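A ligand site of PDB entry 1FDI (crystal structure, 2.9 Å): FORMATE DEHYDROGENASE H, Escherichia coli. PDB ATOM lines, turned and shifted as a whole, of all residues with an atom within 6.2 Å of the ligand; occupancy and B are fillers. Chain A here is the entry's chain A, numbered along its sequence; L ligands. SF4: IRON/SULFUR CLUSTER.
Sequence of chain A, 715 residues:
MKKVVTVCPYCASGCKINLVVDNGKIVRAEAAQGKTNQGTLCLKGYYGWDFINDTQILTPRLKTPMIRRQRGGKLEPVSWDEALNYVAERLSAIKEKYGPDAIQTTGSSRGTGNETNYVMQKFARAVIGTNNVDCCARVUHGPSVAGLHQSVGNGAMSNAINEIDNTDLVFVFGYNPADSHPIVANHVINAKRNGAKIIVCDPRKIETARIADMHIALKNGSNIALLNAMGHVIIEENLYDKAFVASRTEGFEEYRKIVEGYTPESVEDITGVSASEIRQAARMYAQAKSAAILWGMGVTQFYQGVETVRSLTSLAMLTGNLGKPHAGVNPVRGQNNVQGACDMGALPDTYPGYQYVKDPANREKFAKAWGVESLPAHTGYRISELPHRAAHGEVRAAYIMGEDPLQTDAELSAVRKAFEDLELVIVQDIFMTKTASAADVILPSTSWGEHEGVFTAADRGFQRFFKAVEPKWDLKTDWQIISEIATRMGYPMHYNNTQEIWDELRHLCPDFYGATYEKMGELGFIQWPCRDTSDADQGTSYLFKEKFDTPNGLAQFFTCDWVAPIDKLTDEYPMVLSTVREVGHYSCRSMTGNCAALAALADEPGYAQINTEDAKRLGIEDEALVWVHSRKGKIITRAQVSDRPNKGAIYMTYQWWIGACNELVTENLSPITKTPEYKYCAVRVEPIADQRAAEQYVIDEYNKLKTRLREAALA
NZ of Lys 44 lies close to S3 of the ligand (3.7 Å).
An iron atom (FE3) of the ligand is bound by the side-chain sulfur (SG) of Cys 15.
An iron atom (FE2) of the ligand is bound by the side-chain sulfur (SG) of Cys 8 (2.3 Å).
The backbone NH (N) of Gly 14 lies close to a sulfur (S1) of the ligand (3.7 Å).
The backbone NH of Ile 183 sits close to a sulfur (S2) of the ligand (3.6 Å).
N of Cys 42 lies close to S4 of the ligand.
N of Cys 15 lies close to S1 of the ligand (3.6 Å).
S2 of the ligand lies close to OG of Ser 13, at 3.8 Å.
The side-chain sulfur (SG) of Cys 42 binds an iron atom (FE1) of the ligand, 2.4 Å away.
N of Cys 11 sits close to S3 of the ligand, at 3.5 Å.
FE4 of the ligand is bound by SG of Cys 11 (2.3 Å).
Residues that only touch the ligand: Tyr 10 (3.1 Å), Pro 182 (3.6 Å), Gly 45 (3.7 Å) and Leu 41 (3.8 Å).
Hydrophobic or aromatic side chains that line the ligand: Tyr 10, Leu 41, Pro 182 and Ile 183.
Of the 23 residues printed, 12 come within 4 Å of the ligand.
The nearest printed residue that does not touch the ligand is His 181 (4.6 Å).
The side-chain sulfur (SG) of Cys 11 lies close to the backbone carbonyl oxygen (O) of Ser 180, at 3.5 Å.
The backbone carbonyl oxygen (O) of Cys 15 lies within hydrogen-bond range of the backbone NH (N) of Cys 8, at 2.7 Å.
N of Lys 44 lies close to SG of Cys 42 (3.6 Å).
The side-chain sulfur (SG) of Cys 8 sits close to the backbone NH (N) of Tyr 10.
OG of Ser 13 sits close to SG of Cys 11 (2.7 Å).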
ATOM      1  N   CYS A   8      20.110  -0.188 -17.367  1.00  0.00           N
ATOM      2  CA  CYS A   8      21.187   0.776 -17.379  1.00  0.00           C
ATOM      3  C   CYS A   8      22.565   0.131 -17.351  1.00  0.00           C
ATOM      4  O   CYS A   8      22.816  -0.808 -16.575  1.00  0.00           O
ATOM      5  CB  CYS A   8      21.046   1.720 -16.204  1.00  0.00           C
ATOM      6  SG  CYS A   8      22.350   2.982 -16.210  1.00  0.00           S
ATOM      7  N   PRO A   9      23.489   0.633 -18.168  1.00  0.00           N
ATOM      8  CA  PRO A   9      24.857   0.109 -18.244  1.00  0.00           C
ATOM      9  C   PRO A   9      25.864   0.822 -17.331  1.00  0.00           C
ATOM     10  O   PRO A   9      27.086   0.655 -17.468  1.00  0.00           O
ATOM     11  CB  PRO A   9      25.205   0.325 -19.705  1.00  0.00           C
ATOM     12  CG  PRO A   9      24.566   1.645 -19.969  1.00  0.00           C
ATOM     13  CD  PRO A   9      23.222   1.567 -19.263  1.00  0.00           C
ATOM     14  N   TYR A  10      25.370   1.626 -16.402  1.00  0.00           N
ATOM     15  CA  TYR A  10      26.263   2.339 -15.520  1.00  0.00           C
ATOM     16  C   TYR A  10      26.496   1.612 -14.233  1.00  0.00           C
ATOM     17  O   TYR A  10      27.212   0.618 -14.276  1.00  0.00           O
ATOM     18  CB  TYR A  10      25.839   3.797 -15.350  1.00  0.00           C
ATOM     19  CG  TYR A  10      26.019   4.492 -16.657  1.00  0.00           C
ATOM     20  CD1 TYR A  10      27.280   4.859 -17.102  1.00  0.00           C
ATOM     21  CD2 TYR A  10      24.944   4.691 -17.506  1.00  0.00           C
ATOM     22  CE1 TYR A  10      27.472   5.378 -18.363  1.00  0.00           C
ATOM     23  CE2 TYR A  10      25.121   5.214 -18.796  1.00  0.00           C
ATOM     24  CZ  TYR A  10      26.385   5.554 -19.210  1.00  0.00           C
ATOM     25  OH  TYR A  10      26.566   6.051 -20.469  1.00  0.00           O
ATOM     26  N   CYS A  11      25.870   1.990 -13.117  1.00  0.00           N
ATOM     27  CA  CYS A  11      26.143   1.239 -11.918  1.00  0.00           C
ATOM     28  C   CYS A  11      25.425  -0.119 -11.828  1.00  0.00           C
ATOM     29  O   CYS A  11      24.753  -0.541 -12.767  1.00  0.00           O
ATOM     30  CB  CYS A  11      25.971   2.104 -10.679  1.00  0.00           C
ATOM     31  SG  CYS A  11      24.309   2.531 -10.133  1.00  0.00           S
ATOM     32  N   ALA A  12      25.638  -0.837 -10.720  1.00  0.00           N
ATOM     33  CA  ALA A  12      24.981  -2.143 -10.504  1.00  0.00           C
ATOM     34  C   ALA A  12      23.594  -2.071  -9.851  1.00  0.00           C
ATOM     35  O   ALA A  12      23.119  -3.059  -9.285  1.00  0.00           O
ATOM     36  CB  ALA A  12      25.882  -3.031  -9.685  1.00  0.00           C
ATOM     37  N   SER A  13      22.965  -0.897  -9.880  1.00  0.00           N
ATOM     38  CA  SER A  13      21.635  -0.721  -9.291  1.00  0.00           C
ATOM     39  C   SER A  13      20.660  -1.466 -10.172  1.00  0.00           C
ATOM     40  O   SER A  13      19.610  -1.902  -9.714  1.00  0.00           O
ATOM     41  CB  SER A  13      21.275   0.748  -9.213  1.00  0.00           C
ATOM     42  OG  SER A  13      22.328   1.469  -8.583  1.00  0.00           O
ATOM     43  N   GLY A  14      21.009  -1.557 -11.460  1.00  0.00           N
ATOM     44  CA  GLY A  14      20.200  -2.296 -12.415  1.00  0.00           C
ATOM     45  C   GLY A  14      18.855  -1.742 -12.774  1.00  0.00           C
ATOM     46  O   GLY A  14      17.877  -2.493 -12.923  1.00  0.00           O
ATOM     47  N   CYS A  15      18.829  -0.420 -12.934  1.00  0.00           N
ATOM     48  CA  CYS A  15      17.617   0.305 -13.306  1.00  0.00           C
ATOM     49  C   CYS A  15      17.176  -0.081 -14.725  1.00  0.00           C
ATOM     50  O   CYS A  15      17.992  -0.175 -15.643  1.00  0.00           O
ATOM     51  CB  CYS A  15      17.873   1.813 -13.248  1.00  0.00           C
ATOM     52  SG  CYS A  15      18.304   2.474 -11.608  1.00  0.00           S
ATOM     53  N   ILE A  17      15.422   0.711 -18.099  1.00  0.00           N
ATOM     54  CA  ILE A  17      15.217   1.908 -18.899  1.00  0.00           C
ATOM     55  C   ILE A  17      14.331   1.560 -20.100  1.00  0.00           C
ATOM     56  O   ILE A  17      14.305   0.412 -20.549  1.00  0.00           O
ATOM     57  CB  ILE A  17      16.555   2.395 -19.474  1.00  0.00           C
ATOM     58  CG1 ILE A  17      17.470   2.890 -18.378  1.00  0.00           C
ATOM     59  CG2 ILE A  17      16.323   3.463 -20.510  1.00  0.00           C
ATOM     60  CD1 ILE A  17      18.865   3.178 -18.889  1.00  0.00           C
ATOM     61  N   ASN A  37      14.459   0.253  -9.518  1.00  0.00           N
ATOM     62  CA  ASN A  37      14.223   1.691  -9.716  1.00  0.00           C
ATOM     63  C   ASN A  37      12.823   2.192  -9.717  1.00  0.00           C
ATOM     64  O   ASN A  37      12.570   3.297  -9.286  1.00  0.00           O
ATOM     65  CB  ASN A  37      14.899   2.221 -10.978  1.00  0.00           C
ATOM     66  CG  ASN A  37      14.470   1.502 -12.200  1.00  0.00           C
ATOM     67  OD1 ASN A  37      14.420   0.276 -12.187  1.00  0.00           O
ATOM     68  ND2 ASN A  37      14.168   2.241 -13.270  1.00  0.00           N
ATOM     69  N   THR A  40      12.372   5.525 -11.730  1.00  0.00           N
ATOM     70  CA  THR A  40      13.381   6.535 -11.493  1.00  0.00           C
ATOM     71  C   THR A  40      14.726   6.118 -12.064  1.00  0.00           C
ATOM     72  O   THR A  40      14.980   4.938 -12.252  1.00  0.00           O
ATOM     73  CB  THR A  40      13.563   6.777 -10.004  1.00  0.00           C
ATOM     74  OG1 THR A  40      14.404   5.750  -9.457  1.00  0.00           O
ATOM     75  CG2 THR A  40      12.229   6.771  -9.298  1.00  0.00           C
ATOM     76  N   LEU A  41      15.568   7.108 -12.363  1.00  0.00           N
ATOM     77  CA  LEU A  41      16.922   6.913 -12.870  1.00  0.00           C
ATOM     78  C   LEU A  41      17.693   8.139 -12.363  1.00  0.00           C
ATOM     79  O   LEU A  41      17.078   9.128 -11.925  1.00  0.00           O
ATOM     80  CB  LEU A  41      16.979   6.937 -14.399  1.00  0.00           C
ATOM     81  CG  LEU A  41      16.215   5.932 -15.248  1.00  0.00           C
ATOM     82  CD1 LEU A  41      16.418   6.256 -16.738  1.00  0.00           C
ATOM     83  CD2 LEU A  41      16.698   4.503 -14.921  1.00  0.00           C
ATOM     84  N   CYS A  42      19.026   8.081 -12.394  1.00  0.00           N
ATOM     85  CA  CYS A  42      19.828   9.210 -11.976  1.00  0.00           C
ATOM     86  C   CYS A  42      20.209   9.948 -13.259  1.00  0.00           C
ATOM     87  O   CYS A  42      19.739   9.574 -14.332  1.00  0.00           O
ATOM     88  CB  CYS A  42      21.063   8.765 -11.190  1.00  0.00           C
ATOM     89  SG  CYS A  42      22.292   7.939 -12.222  1.00  0.00           S
ATOM     90  N   LEU A  43      21.007  10.992 -13.167  1.00  0.00           N
ATOM     91  CA  LEU A  43      21.416  11.767 -14.332  1.00  0.00           C
ATOM     92  C   LEU A  43      22.041  10.930 -15.474  1.00  0.00           C
ATOM     93  O   LEU A  43      21.767  11.163 -16.658  1.00  0.00           O
ATOM     94  CB  LEU A  43      22.427  12.837 -13.902  1.00  0.00           C
ATOM     95  CG  LEU A  43      22.664  14.098 -14.730  1.00  0.00           C
ATOM     96  CD1 LEU A  43      21.503  15.034 -14.517  1.00  0.00           C
ATOM     97  CD2 LEU A  43      23.966  14.800 -14.261  1.00  0.00           C
ATOM     98  N   LYS A  44      22.849   9.949 -15.118  1.00  0.00           N
ATOM     99  CA  LYS A  44      23.505   9.129 -16.140  1.00  0.00           C
ATOM    100  C   LYS A  44      22.561   8.216 -16.911  1.00  0.00           C
ATOM    101  O   LYS A  44      22.582   8.214 -18.147  1.00  0.00           O
ATOM    102  CB  LYS A  44      24.630   8.295 -15.518  1.00  0.00           C
ATOM    103  CG  LYS A  44      25.906   9.047 -15.204  1.00  0.00           C
ATOM    104  CD  LYS A  44      26.770   8.209 -14.334  1.00  0.00           C
ATOM    105  CE  LYS A  44      25.999   7.877 -13.089  1.00  0.00           C
ATOM    106  NZ  LYS A  44      26.755   7.039 -12.158  1.00  0.00           N
ATOM    107  N   GLY A  45      21.770   7.417 -16.217  1.00  0.00           N
ATOM    108  CA  GLY A  45      20.884   6.549 -16.941  1.00  0.00           C
ATOM    109  C   GLY A  45      19.984   7.344 -17.879  1.00  0.00           C
ATOM    110  O   GLY A  45      19.651   6.876 -18.973  1.00  0.00           O
ATOM    111  N   TYR A  46      19.594   8.550 -17.441  1.00  0.00           N
ATOM    112  CA  TYR A  46      18.703   9.457 -18.191  1.00  0.00           C
ATOM    113  C   TYR A  46      19.370  10.137 -19.368  1.00  0.00           C
ATOM    114  O   TYR A  46      18.767  10.263 -20.422  1.00  0.00           O
ATOM    115  CB  TYR A  46      18.152  10.538 -17.263  1.00  0.00           C
ATOM    116  CG  TYR A  46      16.862  11.215 -17.689  1.00  0.00           C
ATOM    117  CD1 TYR A  46      16.848  12.209 -18.676  1.00  0.00           C
ATOM    118  CD2 TYR A  46      15.669  10.854 -17.087  1.00  0.00           C
ATOM    119  CE1 TYR A  46      15.635  12.841 -19.054  1.00  0.00           C
ATOM    120  CE2 TYR A  46      14.472  11.472 -17.433  1.00  0.00           C
ATOM    121  CZ  TYR A  46      14.452  12.466 -18.413  1.00  0.00           C
ATOM    122  OH  TYR A  46      13.231  13.090 -18.669  1.00  0.00           O
ATOM    123  N   SER A 180      27.652   6.528  -5.717  1.00  0.00           N
ATOM    124  CA  SER A 180      27.902   5.283  -6.419  1.00  0.00           C
ATOM    125  C   SER A 180      26.699   4.547  -6.974  1.00  0.00           C
ATOM    126  O   SER A 180      26.746   4.074  -8.077  1.00  0.00           O
ATOM    127  CB  SER A 180      28.708   4.356  -5.542  1.00  0.00           C
ATOM    128  OG  SER A 180      29.881   5.020  -5.151  1.00  0.00           O
ATOM    129  N   HIS A 181      25.663   4.363  -6.170  1.00  0.00           N
ATOM    130  CA  HIS A 181      24.457   3.685  -6.652  1.00  0.00           C
ATOM    131  C   HIS A 181      23.252   4.550  -6.171  1.00  0.00           C
ATOM    132  O   HIS A 181      22.636   4.259  -5.138  1.00  0.00           O
ATOM    133  CB  HIS A 181      24.395   2.242  -6.071  1.00  0.00           C
ATOM    134  CG  HIS A 181      25.639   1.421  -6.279  1.00  0.00           C
ATOM    135  ND1 HIS A 181      26.620   1.311  -5.320  1.00  0.00           N
ATOM    136  CD2 HIS A 181      26.079   0.706  -7.346  1.00  0.00           C
ATOM    137  CE1 HIS A 181      27.618   0.579  -5.793  1.00  0.00           C
ATOM    138  NE2 HIS A 181      27.309   0.203  -7.017  1.00  0.00           N
ATOM    139  N   PRO A 182      22.926   5.647  -6.886  1.00  0.00           N
ATOM    140  CA  PRO A 182      21.821   6.526  -6.517  1.00  0.00           C
ATOM    141  C   PRO A 182      20.511   5.836  -6.169  1.00  0.00           C
ATOM    142  O   PRO A 182      19.836   6.221  -5.205  1.00  0.00           O
ATOM    143  CB  PRO A 182      21.696   7.429  -7.726  1.00  0.00           C
ATOM    144  CG  PRO A 182      23.098   7.610  -8.105  1.00  0.00           C
ATOM    145  CD  PRO A 182      23.660   6.209  -8.028  1.00  0.00           C
ATOM    146  N   ILE A 183      20.118   4.831  -6.964  1.00  0.00           N
ATOM    147  CA  ILE A 183      18.891   4.076  -6.693  1.00  0.00           C
ATOM    148  C   ILE A 183      19.067   3.248  -5.412  1.00  0.00           C
ATOM    149  O   ILE A 183      18.095   2.981  -4.719  1.00  0.00           O
ATOM    150  CB  ILE A 183      18.490   3.168  -7.910  1.00  0.00           C
ATOM    151  CG1 ILE A 183      17.466   3.887  -8.809  1.00  0.00           C
ATOM    152  CG2 ILE A 183      17.907   1.827  -7.447  1.00  0.00           C
ATOM    153  CD1 ILE A 183      17.884   5.288  -9.339  1.00  0.00           C
ATOM    154  N   VAL A 184      20.289   2.845  -5.085  1.00  0.00           N
ATOM    155  CA  VAL A 184      20.540   2.096  -3.852  1.00  0.00           C
ATOM    156  C   VAL A 184      20.484   3.149  -2.728  1.00  0.00           C
ATOM    157  O   VAL A 184      19.962   2.889  -1.624  1.00  0.00           O
ATOM    158  CB  VAL A 184      21.921   1.294  -3.872  1.00  0.00           C
ATOM    159  CG1 VAL A 184      22.278   0.779  -2.488  1.00  0.00           C
ATOM    160  CG2 VAL A 184      21.827   0.078  -4.786  1.00  0.00           C
ATOM    161  N   TYR A 586      31.311   8.167 -15.241  1.00  0.00           N
ATOM    162  CA  TYR A 586      31.467   6.807 -14.761  1.00  0.00           C
ATOM    163  C   TYR A 586      32.695   6.022 -15.186  1.00  0.00           C
ATOM    164  O   TYR A 586      32.799   5.595 -16.328  1.00  0.00           O
ATOM    165  CB  TYR A 586      30.183   6.013 -15.071  1.00  0.00           C
ATOM    166  CG  TYR A 586      30.208   4.618 -14.542  1.00  0.00           C
ATOM    167  CD1 TYR A 586      30.928   3.621 -15.203  1.00  0.00           C
ATOM    168  CD2 TYR A 586      29.559   4.287 -13.356  1.00  0.00           C
ATOM    169  CE1 TYR A 586      31.016   2.325 -14.689  1.00  0.00           C
ATOM    170  CE2 TYR A 586      29.637   2.969 -12.840  1.00  0.00           C
ATOM    171  CZ  TYR A 586      30.371   2.023 -13.527  1.00  0.00           C
ATOM    172  OH  TYR A 586      30.511   0.764 -13.029  1.00  0.00           O
HETATM  173 FE1  SF4 L   1      21.929   5.574 -12.249  1.00  0.00          FE
HETATM  174 FE2  SF4 L   1      22.162   3.664 -14.058  1.00  0.00          FE
HETATM  175 FE3  SF4 L   1      20.329   3.365 -12.024  1.00  0.00          FE
HETATM  176 FE4  SF4 L   1      22.788   3.479 -11.639  1.00  0.00          FE
HETATM  177  S1  SF4 L   1      21.699   1.833 -12.904  1.00  0.00           S
HETATM  178  S2  SF4 L   1      21.345   4.647 -10.334  1.00  0.00           S
HETATM  179  S3  SF4 L   1      23.885   4.848 -13.168  1.00  0.00           S
HETATM  180  S4  SF4 L   1      20.235   4.912 -13.643  1.00  0.00           S
